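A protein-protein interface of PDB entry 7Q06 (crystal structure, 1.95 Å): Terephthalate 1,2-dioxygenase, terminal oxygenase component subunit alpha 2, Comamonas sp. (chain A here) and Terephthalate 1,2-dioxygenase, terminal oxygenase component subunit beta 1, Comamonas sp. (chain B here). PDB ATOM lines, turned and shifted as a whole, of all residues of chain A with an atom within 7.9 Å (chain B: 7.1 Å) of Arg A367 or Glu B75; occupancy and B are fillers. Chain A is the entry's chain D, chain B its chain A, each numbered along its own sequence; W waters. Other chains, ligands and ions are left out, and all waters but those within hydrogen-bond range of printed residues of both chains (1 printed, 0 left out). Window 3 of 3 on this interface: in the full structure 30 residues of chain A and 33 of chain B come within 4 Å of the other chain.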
ATOM      1  N   PRO A 197     -14.027   1.210 -26.801  1.00  0.00           N
ATOM      2  CA  PRO A 197     -13.732   2.328 -27.711  1.00  0.00           C
ATOM      3  C   PRO A 197     -13.437   3.604 -26.871  1.00  0.00           C
ATOM      4  O   PRO A 197     -14.112   4.634 -27.025  1.00  0.00           O
ATOM      5  CB  PRO A 197     -15.083   2.474 -28.462  1.00  0.00           C
ATOM      6  CG  PRO A 197     -16.078   2.216 -27.355  1.00  0.00           C
ATOM      7  CD  PRO A 197     -15.479   1.042 -26.607  1.00  0.00           C
ATOM      8  N   ASN A 198     -12.482   3.521 -25.938  1.00  0.00           N
ATOM      9  CA  ASN A 198     -12.143   4.673 -25.065  1.00  0.00           C
ATOM     10  C   ASN A 198     -10.721   4.498 -24.557  1.00  0.00           C
ATOM     11  O   ASN A 198     -10.200   3.352 -24.498  1.00  0.00           O
ATOM     12  CB  ASN A 198     -13.154   4.860 -23.936  1.00  0.00           C
ATOM     13  CG  ASN A 198     -13.399   3.607 -23.127  1.00  0.00           C
ATOM     14  OD1 ASN A 198     -14.390   2.918 -23.306  1.00  0.00           O
ATOM     15  ND2 ASN A 198     -12.475   3.260 -22.261  1.00  0.00           N
ATOM     16  N   LEU A 202     -10.684   6.142 -18.817  1.00  0.00           N
ATOM     17  CA  LEU A 202     -12.156   6.273 -18.670  1.00  0.00           C
ATOM     18  C   LEU A 202     -12.761   4.979 -18.102  1.00  0.00           C
ATOM     19  O   LEU A 202     -13.703   5.096 -17.334  1.00  0.00           O
ATOM     20  CB  LEU A 202     -12.781   6.638 -20.019  1.00  0.00           C
ATOM     21  CG  LEU A 202     -12.478   8.077 -20.440  1.00  0.00           C
ATOM     22  CD1 LEU A 202     -12.906   8.326 -21.873  1.00  0.00           C
ATOM     23  CD2 LEU A 202     -13.169   9.056 -19.484  1.00  0.00           C
ATOM     24  N   MET A 356     -22.514  -4.532 -19.646  1.00  0.00           N
ATOM     25  CA  MET A 356     -22.622  -4.115 -21.067  1.00  0.00           C
ATOM     26  C   MET A 356     -22.569  -2.582 -21.083  1.00  0.00           C
ATOM     27  O   MET A 356     -21.863  -2.070 -21.885  1.00  0.00           O
ATOM     28  CB  MET A 356     -23.856  -4.673 -21.806  1.00  0.00           C
ATOM     29  CG  MET A 356     -25.187  -4.034 -21.542  1.00  0.00           C
ATOM     30  SD  MET A 356     -26.387  -4.557 -22.794  1.00  0.00           S
ATOM     31  CE  MET A 356     -26.642  -6.275 -22.384  1.00  0.00           C
ATOM     32  N   ALA A 360     -19.862   0.686 -22.876  1.00  0.00           N
ATOM     33  CA  ALA A 360     -20.307   1.770 -23.775  1.00  0.00           C
ATOM     34  C   ALA A 360     -20.070   3.190 -23.195  1.00  0.00           C
ATOM     35  O   ALA A 360     -19.799   4.111 -24.040  1.00  0.00           O
ATOM     36  CB  ALA A 360     -21.780   1.585 -24.086  1.00  0.00           C
ATOM     37  N   VAL A 361     -20.201   3.378 -21.862  1.00  0.00           N
ATOM     38  CA  VAL A 361     -20.220   4.743 -21.281  1.00  0.00           C
ATOM     39  C   VAL A 361     -18.886   5.412 -21.551  1.00  0.00           C
ATOM     40  O   VAL A 361     -18.921   6.617 -21.746  1.00  0.00           O
ATOM     41  CB  VAL A 361     -20.587   4.872 -19.798  1.00  0.00           C
ATOM     42  CG1 VAL A 361     -22.030   4.552 -19.614  1.00  0.00           C
ATOM     43  CG2 VAL A 361     -19.684   4.079 -18.862  1.00  0.00           C
ATOM     44  N   GLY A 362     -17.775   4.676 -21.484  1.00  0.00           N
ATOM     45  CA  GLY A 362     -16.460   5.253 -21.776  1.00  0.00           C
ATOM     46  C   GLY A 362     -16.439   5.947 -23.143  1.00  0.00           C
ATOM     47  O   GLY A 362     -15.918   7.086 -23.290  1.00  0.00           O
ATOM     48  N   GLY A 363     -16.992   5.280 -24.132  1.00  0.00           N
ATOM     49  CA  GLY A 363     -17.057   5.797 -25.510  1.00  0.00           C
ATOM     50  C   GLY A 363     -17.965   7.006 -25.571  1.00  0.00           C
ATOM     51  O   GLY A 363     -17.673   7.917 -26.333  1.00  0.00           O
ATOM     52  N   PHE A 364     -19.037   7.033 -24.800  1.00  0.00           N
ATOM     53  CA  PHE A 364     -19.954   8.196 -24.772  1.00  0.00           C
ATOM     54  C   PHE A 364     -19.153   9.398 -24.276  1.00  0.00           C
ATOM     55  O   PHE A 364     -19.392  10.484 -24.810  1.00  0.00           O
ATOM     56  CB  PHE A 364     -21.193   7.923 -23.932  1.00  0.00           C
ATOM     57  CG  PHE A 364     -22.053   6.786 -24.438  1.00  0.00           C
ATOM     58  CD1 PHE A 364     -21.987   6.353 -25.746  1.00  0.00           C
ATOM     59  CD2 PHE A 364     -22.961   6.192 -23.591  1.00  0.00           C
ATOM     60  CE1 PHE A 364     -22.828   5.355 -26.209  1.00  0.00           C
ATOM     61  CE2 PHE A 364     -23.803   5.184 -24.046  1.00  0.00           C
ATOM     62  CZ  PHE A 364     -23.713   4.753 -25.348  1.00  0.00           C
ATOM     63  N   VAL A 365     -18.232   9.208 -23.329  1.00  0.00           N
ATOM     64  CA  VAL A 365     -17.378  10.321 -22.833  1.00  0.00           C
ATOM     65  C   VAL A 365     -16.391  10.704 -23.953  1.00  0.00           C
ATOM     66  O   VAL A 365     -16.258  11.927 -24.323  1.00  0.00           O
ATOM     67  CB  VAL A 365     -16.674   9.964 -21.503  1.00  0.00           C
ATOM     68  CG1 VAL A 365     -15.751  11.103 -21.053  1.00  0.00           C
ATOM     69  CG2 VAL A 365     -17.703   9.677 -20.408  1.00  0.00           C
ATOM     70  N   GLN A 366     -15.687   9.714 -24.487  1.00  0.00           N
ATOM     71  CA  GLN A 366     -14.654   9.962 -25.538  1.00  0.00           C
ATOM     72  C   GLN A 366     -15.282  10.822 -26.640  1.00  0.00           C
ATOM     73  O   GLN A 366     -14.659  11.773 -27.085  1.00  0.00           O
ATOM     74  CB  GLN A 366     -14.097   8.617 -26.036  1.00  0.00           C
ATOM     75  CG  GLN A 366     -12.804   8.738 -26.840  1.00  0.00           C
ATOM     76  CD  GLN A 366     -11.562   8.759 -25.966  1.00  0.00           C
ATOM     77  OE1 GLN A 366     -11.446   8.032 -24.969  1.00  0.00           O
ATOM     78  NE2 GLN A 366     -10.611   9.619 -26.325  1.00  0.00           N
ATOM     79  N   ARG A 367     -16.519  10.534 -27.035  1.00  0.00           N
ATOM     80  CA  ARG A 367     -17.205  11.245 -28.119  1.00  0.00           C
ATOM     81  C   ARG A 367     -17.800  12.554 -27.625  1.00  0.00           C
ATOM     82  O   ARG A 367     -17.800  13.573 -28.412  1.00  0.00           O
ATOM     83  CB  ARG A 367     -18.262  10.348 -28.740  1.00  0.00           C
ATOM     84  CG  ARG A 367     -17.660   9.313 -29.683  1.00  0.00           C
ATOM     85  CD  ARG A 367     -18.478   8.041 -29.865  1.00  0.00           C
ATOM     86  NE  ARG A 367     -19.784   8.376 -30.407  1.00  0.00           N
ATOM     87  CZ  ARG A 367     -20.797   7.536 -30.460  1.00  0.00           C
ATOM     88  NH1 ARG A 367     -21.968   7.899 -30.976  1.00  0.00           N
ATOM     89  NH2 ARG A 367     -20.664   6.363 -29.878  1.00  0.00           N
ATOM     90  N   GLY A 368     -18.365  12.564 -26.428  1.00  0.00           N
ATOM     91  CA  GLY A 368     -18.972  13.766 -25.872  1.00  0.00           C
ATOM     92  C   GLY A 368     -17.986  14.934 -25.737  1.00  0.00           C
ATOM     93  O   GLY A 368     -18.421  16.117 -25.804  1.00  0.00           O
ATOM     94  N   ILE A 369     -16.704  14.651 -25.550  1.00  0.00           N
ATOM     95  CA  ILE A 369     -15.669  15.689 -25.315  1.00  0.00           C
ATOM     96  C   ILE A 369     -14.980  16.061 -26.632  1.00  0.00           C
ATOM     97  O   ILE A 369     -13.964  16.771 -26.566  1.00  0.00           O
ATOM     98  CB  ILE A 369     -14.654  15.243 -24.244  1.00  0.00           C
ATOM     99  CG1 ILE A 369     -13.821  14.030 -24.680  1.00  0.00           C
ATOM    100  CG2 ILE A 369     -15.376  15.022 -22.920  1.00  0.00           C
ATOM    101  CD1 ILE A 369     -12.812  13.566 -23.666  1.00  0.00           C
ATOM    102  N   ALA A 370     -15.448  15.586 -27.781  1.00  0.00           N
ATOM    103  CA  ALA A 370     -14.681  15.721 -29.057  1.00  0.00           C
ATOM    104  C   ALA A 370     -14.406  17.207 -29.350  1.00  0.00           C
ATOM    105  O   ALA A 370     -13.362  17.484 -29.921  1.00  0.00           O
ATOM    106  CB  ALA A 370     -15.428  15.037 -30.196  1.00  0.00           C
ATOM    107  N   GLY A 371     -15.311  18.141 -29.009  1.00  0.00           N
ATOM    108  CA  GLY A 371     -15.059  19.594 -29.174  1.00  0.00           C
ATOM    109  C   GLY A 371     -14.541  20.325 -27.942  1.00  0.00           C
ATOM    110  O   GLY A 371     -14.657  21.572 -27.895  1.00  0.00           O
ATOM    111  N   ALA A 372     -14.059  19.615 -26.924  1.00  0.00           N
ATOM    112  CA  ALA A 372     -13.894  20.169 -25.560  1.00  0.00           C
ATOM    113  C   ALA A 372     -12.516  19.787 -24.987  1.00  0.00           C
ATOM    114  O   ALA A 372     -12.412  19.713 -23.755  1.00  0.00           O
ATOM    115  CB  ALA A 372     -15.013  19.665 -24.668  1.00  0.00           C
ATOM    116  N   ILE B  73     -28.917   0.021 -21.303  1.00  0.00           N
ATOM    117  CA  ILE B  73     -28.381   1.222 -22.013  1.00  0.00           C
ATOM    118  C   ILE B  73     -27.320   0.696 -22.994  1.00  0.00           C
ATOM    119  O   ILE B  73     -26.301   0.066 -22.571  1.00  0.00           O
ATOM    120  CB  ILE B  73     -27.778   2.263 -21.044  1.00  0.00           C
ATOM    121  CG1 ILE B  73     -28.833   2.949 -20.166  1.00  0.00           C
ATOM    122  CG2 ILE B  73     -26.912   3.270 -21.810  1.00  0.00           C
ATOM    123  CD1 ILE B  73     -30.106   3.328 -20.899  1.00  0.00           C
ATOM    124  N   TYR B  74     -27.582   0.884 -24.282  1.00  0.00           N
ATOM    125  CA  TYR B  74     -26.586   0.578 -25.347  1.00  0.00           C
ATOM    126  C   TYR B  74     -26.938   1.487 -26.529  1.00  0.00           C
ATOM    127  O   TYR B  74     -28.105   1.886 -26.675  1.00  0.00           O
ATOM    128  CB  TYR B  74     -26.591  -0.930 -25.639  1.00  0.00           C
ATOM    129  CG  TYR B  74     -27.945  -1.405 -26.096  1.00  0.00           C
ATOM    130  CD1 TYR B  74     -28.314  -1.392 -27.446  1.00  0.00           C
ATOM    131  CD2 TYR B  74     -28.903  -1.820 -25.177  1.00  0.00           C
ATOM    132  CE1 TYR B  74     -29.557  -1.878 -27.869  1.00  0.00           C
ATOM    133  CE2 TYR B  74     -30.168  -2.251 -25.575  1.00  0.00           C
ATOM    134  CZ  TYR B  74     -30.487  -2.300 -26.926  1.00  0.00           C
ATOM    135  OH  TYR B  74     -31.740  -2.690 -27.263  1.00  0.00           O
ATOM    136  N   GLU B  75     -25.936   1.790 -27.342  1.00  0.00           N
ATOM    137  CA  GLU B  75     -26.162   2.588 -28.555  1.00  0.00           C
ATOM    138  C   GLU B  75     -26.933   1.720 -29.589  1.00  0.00           C
ATOM    139  O   GLU B  75     -26.583   0.526 -29.772  1.00  0.00           O
ATOM    140  CB  GLU B  75     -24.809   3.098 -29.032  1.00  0.00           C
ATOM    141  CG  GLU B  75     -24.979   4.293 -29.933  1.00  0.00           C
ATOM    142  CD  GLU B  75     -23.707   4.905 -30.437  1.00  0.00           C
ATOM    143  OE1 GLU B  75     -22.623   4.423 -30.087  1.00  0.00           O
ATOM    144  OE2 GLU B  75     -23.818   5.831 -31.266  1.00  0.00           O
ATOM    145  N   ARG B  76     -27.924   2.305 -30.247  1.00  0.00           N
ATOM    146  CA  ARG B  76     -28.748   1.654 -31.295  1.00  0.00           C
ATOM    147  C   ARG B  76     -27.883   1.028 -32.396  1.00  0.00           C
ATOM    148  O   ARG B  76     -26.988   1.668 -32.953  1.00  0.00           O
ATOM    149  CB  ARG B  76     -29.775   2.634 -31.818  1.00  0.00           C
ATOM    150  CG  ARG B  76     -30.700   2.074 -32.893  1.00  0.00           C
ATOM    151  CD  ARG B  76     -31.894   2.979 -33.194  1.00  0.00           C
ATOM    152  NE  ARG B  76     -32.519   3.267 -31.893  1.00  0.00           N
ATOM    153  CZ  ARG B  76     -33.509   2.550 -31.363  1.00  0.00           C
ATOM    154  NH1 ARG B  76     -34.054   1.554 -32.061  1.00  0.00           N
ATOM    155  NH2 ARG B  76     -33.953   2.841 -30.150  1.00  0.00           N
ATOM    156  N   HIS B  77     -28.149  -0.240 -32.694  1.00  0.00           N
ATOM    157  CA  HIS B  77     -27.453  -0.948 -33.784  1.00  0.00           C
ATOM    158  C   HIS B  77     -28.336  -2.082 -34.228  1.00  0.00           C
ATOM    159  O   HIS B  77     -29.270  -2.391 -33.512  1.00  0.00           O
ATOM    160  CB  HIS B  77     -26.054  -1.420 -33.371  1.00  0.00           C
ATOM    161  CG  HIS B  77     -26.028  -2.392 -32.229  1.00  0.00           C
ATOM    162  ND1 HIS B  77     -26.113  -1.984 -30.894  1.00  0.00           N
ATOM    163  CD2 HIS B  77     -25.924  -3.747 -32.206  1.00  0.00           C
ATOM    164  CE1 HIS B  77     -25.991  -3.032 -30.116  1.00  0.00           C
ATOM    165  NE2 HIS B  77     -25.867  -4.122 -30.890  1.00  0.00           N
ATOM    166  N   ARG B  78     -27.979  -2.675 -35.358  1.00  0.00           N
ATOM    167  CA  ARG B  78     -28.706  -3.830 -35.931  1.00  0.00           C
ATOM    168  C   ARG B  78     -27.689  -4.879 -36.337  1.00  0.00           C
ATOM    169  O   ARG B  78     -26.502  -4.533 -36.552  1.00  0.00           O
ATOM    170  CB  ARG B  78     -29.499  -3.367 -37.165  1.00  0.00           C
ATOM    171  CG  ARG B  78     -30.581  -2.329 -36.872  1.00  0.00           C
ATOM    172  CD  ARG B  78     -31.829  -2.790 -36.110  1.00  0.00           C
ATOM    173  NE  ARG B  78     -32.746  -3.639 -36.880  1.00  0.00           N
ATOM    174  CZ  ARG B  78     -33.398  -3.287 -38.001  1.00  0.00           C
ATOM    175  NH1 ARG B  78     -33.321  -2.047 -38.503  1.00  0.00           N
ATOM    176  NH2 ARG B  78     -34.149  -4.210 -38.588  1.00  0.00           N
ATOM    177  N   ARG B 106     -22.419  -5.992 -37.586  1.00  0.00           N
ATOM    178  CA  ARG B 106     -23.087  -4.977 -36.755  1.00  0.00           C
ATOM    179  C   ARG B 106     -23.085  -3.653 -37.524  1.00  0.00           C
ATOM    180  O   ARG B 106     -22.031  -3.216 -38.036  1.00  0.00           O
ATOM    181  CB  ARG B 106     -22.365  -4.777 -35.426  1.00  0.00           C
ATOM    182  CG  ARG B 106     -23.039  -3.751 -34.534  1.00  0.00           C
ATOM    183  CD  ARG B 106     -22.281  -3.486 -33.262  1.00  0.00           C
ATOM    184  NE  ARG B 106     -20.998  -2.856 -33.545  1.00  0.00           N
ATOM    185  CZ  ARG B 106     -19.969  -2.844 -32.685  1.00  0.00           C
ATOM    186  NH1 ARG B 106     -18.856  -2.246 -32.999  1.00  0.00           N
ATOM    187  NH2 ARG B 106     -20.074  -3.384 -31.480  1.00  0.00           N
ATOM    188  N   MET B 108     -24.083   0.150 -36.829  1.00  0.00           N
ATOM    189  CA  MET B 108     -24.467   1.199 -35.863  1.00  0.00           C
ATOM    190  C   MET B 108     -25.531   2.085 -36.533  1.00  0.00           C
ATOM    191  O   MET B 108     -25.509   2.259 -37.813  1.00  0.00           O
ATOM    192  CB  MET B 108     -23.247   2.019 -35.451  1.00  0.00           C
ATOM    193  CG  MET B 108     -22.076   1.213 -34.826  1.00  0.00           C
ATOM    194  SD  MET B 108     -22.654   0.168 -33.437  1.00  0.00           S
ATOM    195  CE  MET B 108     -23.289   1.355 -32.229  1.00  0.00           C
ATOM    196  N   HIS B 109     -26.415   2.687 -35.743  1.00  0.00           N
ATOM    197  CA  HIS B 109     -27.385   3.710 -36.231  1.00  0.00           C
ATOM    198  C   HIS B 109     -26.645   4.859 -36.965  1.00  0.00           C
ATOM    199  O   HIS B 109     -27.251   5.478 -37.826  1.00  0.00           O
ATOM    200  CB  HIS B 109     -28.275   4.163 -35.053  1.00  0.00           C
ATOM    201  CG  HIS B 109     -27.534   4.996 -34.033  1.00  0.00           C
ATOM    202  ND1 HIS B 109     -28.127   6.082 -33.434  1.00  0.00           N
ATOM    203  CD2 HIS B 109     -26.305   4.860 -33.464  1.00  0.00           C
ATOM    204  CE1 HIS B 109     -27.281   6.612 -32.553  1.00  0.00           C
ATOM    205  NE2 HIS B 109     -26.152   5.886 -32.560  1.00  0.00           N
ATOM    206  N   THR B 110     -25.380   5.113 -36.643  1.00  0.00           N
ATOM    207  CA  THR B 110     -24.525   6.148 -37.264  1.00  0.00           C
ATOM    208  C   THR B 110     -23.876   5.662 -38.573  1.00  0.00           C
ATOM    209  O   THR B 110     -23.163   6.452 -39.200  1.00  0.00           O
ATOM    210  CB  THR B 110     -23.502   6.661 -36.260  1.00  0.00           C
ATOM    211  OG1 THR B 110     -22.857   5.543 -35.644  1.00  0.00           O
ATOM    212  CG2 THR B 110     -24.163   7.562 -35.228  1.00  0.00           C
ATOM    213  N   GLU B 112     -21.707   2.855 -39.393  1.00  0.00           N
ATOM    214  CA  GLU B 112     -20.485   2.009 -39.441  1.00  0.00           C
ATOM    215  C   GLU B 112     -20.937   0.551 -39.522  1.00  0.00           C
ATOM    216  O   GLU B 112     -21.801   0.104 -38.680  1.00  0.00           O
ATOM    217  CB  GLU B 112     -19.561   2.253 -38.226  1.00  0.00           C
ATOM    218  CG  GLU B 112     -19.055   3.716 -38.054  1.00  0.00           C
ATOM    219  CD  GLU B 112     -19.968   4.622 -37.225  1.00  0.00           C
ATOM    220  OE1 GLU B 112     -21.204   4.370 -37.081  1.00  0.00           O
ATOM    221  OE2 GLU B 112     -19.473   5.656 -36.772  1.00  0.00           O
ATOM    222  N   THR B 148     -16.918  -3.534 -27.917  1.00  0.00           N
ATOM    223  CA  THR B 148     -17.719  -2.653 -27.048  1.00  0.00           C
ATOM    224  C   THR B 148     -18.612  -3.444 -26.104  1.00  0.00           C
ATOM    225  O   THR B 148     -18.414  -3.375 -24.875  1.00  0.00           O
ATOM    226  CB  THR B 148     -18.573  -1.657 -27.848  1.00  0.00           C
ATOM    227  OG1 THR B 148     -17.671  -0.979 -28.715  1.00  0.00           O
ATOM    228  CG2 THR B 148     -19.277  -0.654 -26.954  1.00  0.00           C
ATOM    229  N   LEU B 149     -19.580  -4.154 -26.619  1.00  0.00           N
ATOM    230  CA  LEU B 149     -20.553  -4.939 -25.817  1.00  0.00           C
ATOM    231  C   LEU B 149     -21.344  -5.841 -26.787  1.00  0.00           C
ATOM    232  O   LEU B 149     -21.232  -5.659 -28.002  1.00  0.00           O
ATOM    233  CB  LEU B 149     -21.522  -4.004 -25.077  1.00  0.00           C
ATOM    234  CG  LEU B 149     -22.309  -2.996 -25.956  1.00  0.00           C
ATOM    235  CD1 LEU B 149     -23.523  -3.618 -26.577  1.00  0.00           C
ATOM    236  CD2 LEU B 149     -22.742  -1.774 -25.154  1.00  0.00           C
ATOM    237  N   ALA B 151     -25.375  -6.759 -27.062  1.00  0.00           N
ATOM    238  CA  ALA B 151     -26.748  -6.543 -26.549  1.00  0.00           C
ATOM    239  C   ALA B 151     -27.672  -7.593 -27.157  1.00  0.00           C
ATOM    240  O   ALA B 151     -28.450  -8.193 -26.437  1.00  0.00           O
ATOM    241  CB  ALA B 151     -27.216  -5.146 -26.863  1.00  0.00           C
HETATM  242  O   HOH W   1     -21.975   5.264 -33.201  1.00  0.00           O
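NH2 of Arg A367 is in salt-bridge range of OE1 of Glu B75 (2.8 Å).
Water W1 lies within hydrogen-bond range of the side-chain hydroxyl (OG1) of Thr B110 (2.6 Å), the side-chain carboxylate (OE2) of Glu B75 (2.7 Å) and the guanidinium group (NH1) of Arg A367 (3.4 Å).
Of the 14 printed residues of chain B, 3 touch a printed residue of chain A.
Printed residues of chain B that touch a printed residue of chain A: Glu B75, Thr B148 and Leu B149.
Hydrophobic or aromatic side chains of chain B within 4 Å of the printed part of chain A: Leu B149.
Along chain A the printed residues that touch a printed residue of chain B span positions 197 to 367.
Among the printed residues, 5 pairs touch across the chains.
Among the printed residues, Asp or Glu carboxylates within 4 Å of a Lys or Arg side-chain nitrogen of the other chain: Arg A367 with Glu B75.
Of chain B, only Glu B75 (2.8 Å) comes within 4 Å of Arg A367.
Printed residues of chain A within 4 Å of Glu B75: Phe A364 (3.99 Å) and Arg A367 (2.8 Å).
Printed residues of chain A within 4 Å of Leu B149: Met A356 (3.4 Å) and Ala A360 (3.7 Å).
Printed residues of chain B within 4 Å of Phe A364: Glu B75 (3.99 Å).
Printed residues of chain B within 4 Å of Pro A197: Thr B148.
Printed residues of chain A within 4 Å of Thr B148: Pro A197 (3.7 Å).
The nearest printed residue of chain A that does not touch Glu B75 is Ala A360 (5.3 Å).
The nearest printed residue of chain B that does not touch Pro A197 is Leu B149 (6.6 Å).
Thr B148 touches Pro A197.
Leu B149 touches Met A356 (CD2 to O, 3.4 Å).
CB of Ala A360 touches CD2 of Leu B149, at 3.7 Å.
Phe A364 touches Glu B75.
ND1 of His B77 lies within hydrogen-bond range of O of Glu B75, at 2.8 Å.
The side-chain carboxylate of Glu B75 sits at hydrogen-bond distance from a ring nitrogen (NE2) of His B109, 2.7 Å away.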
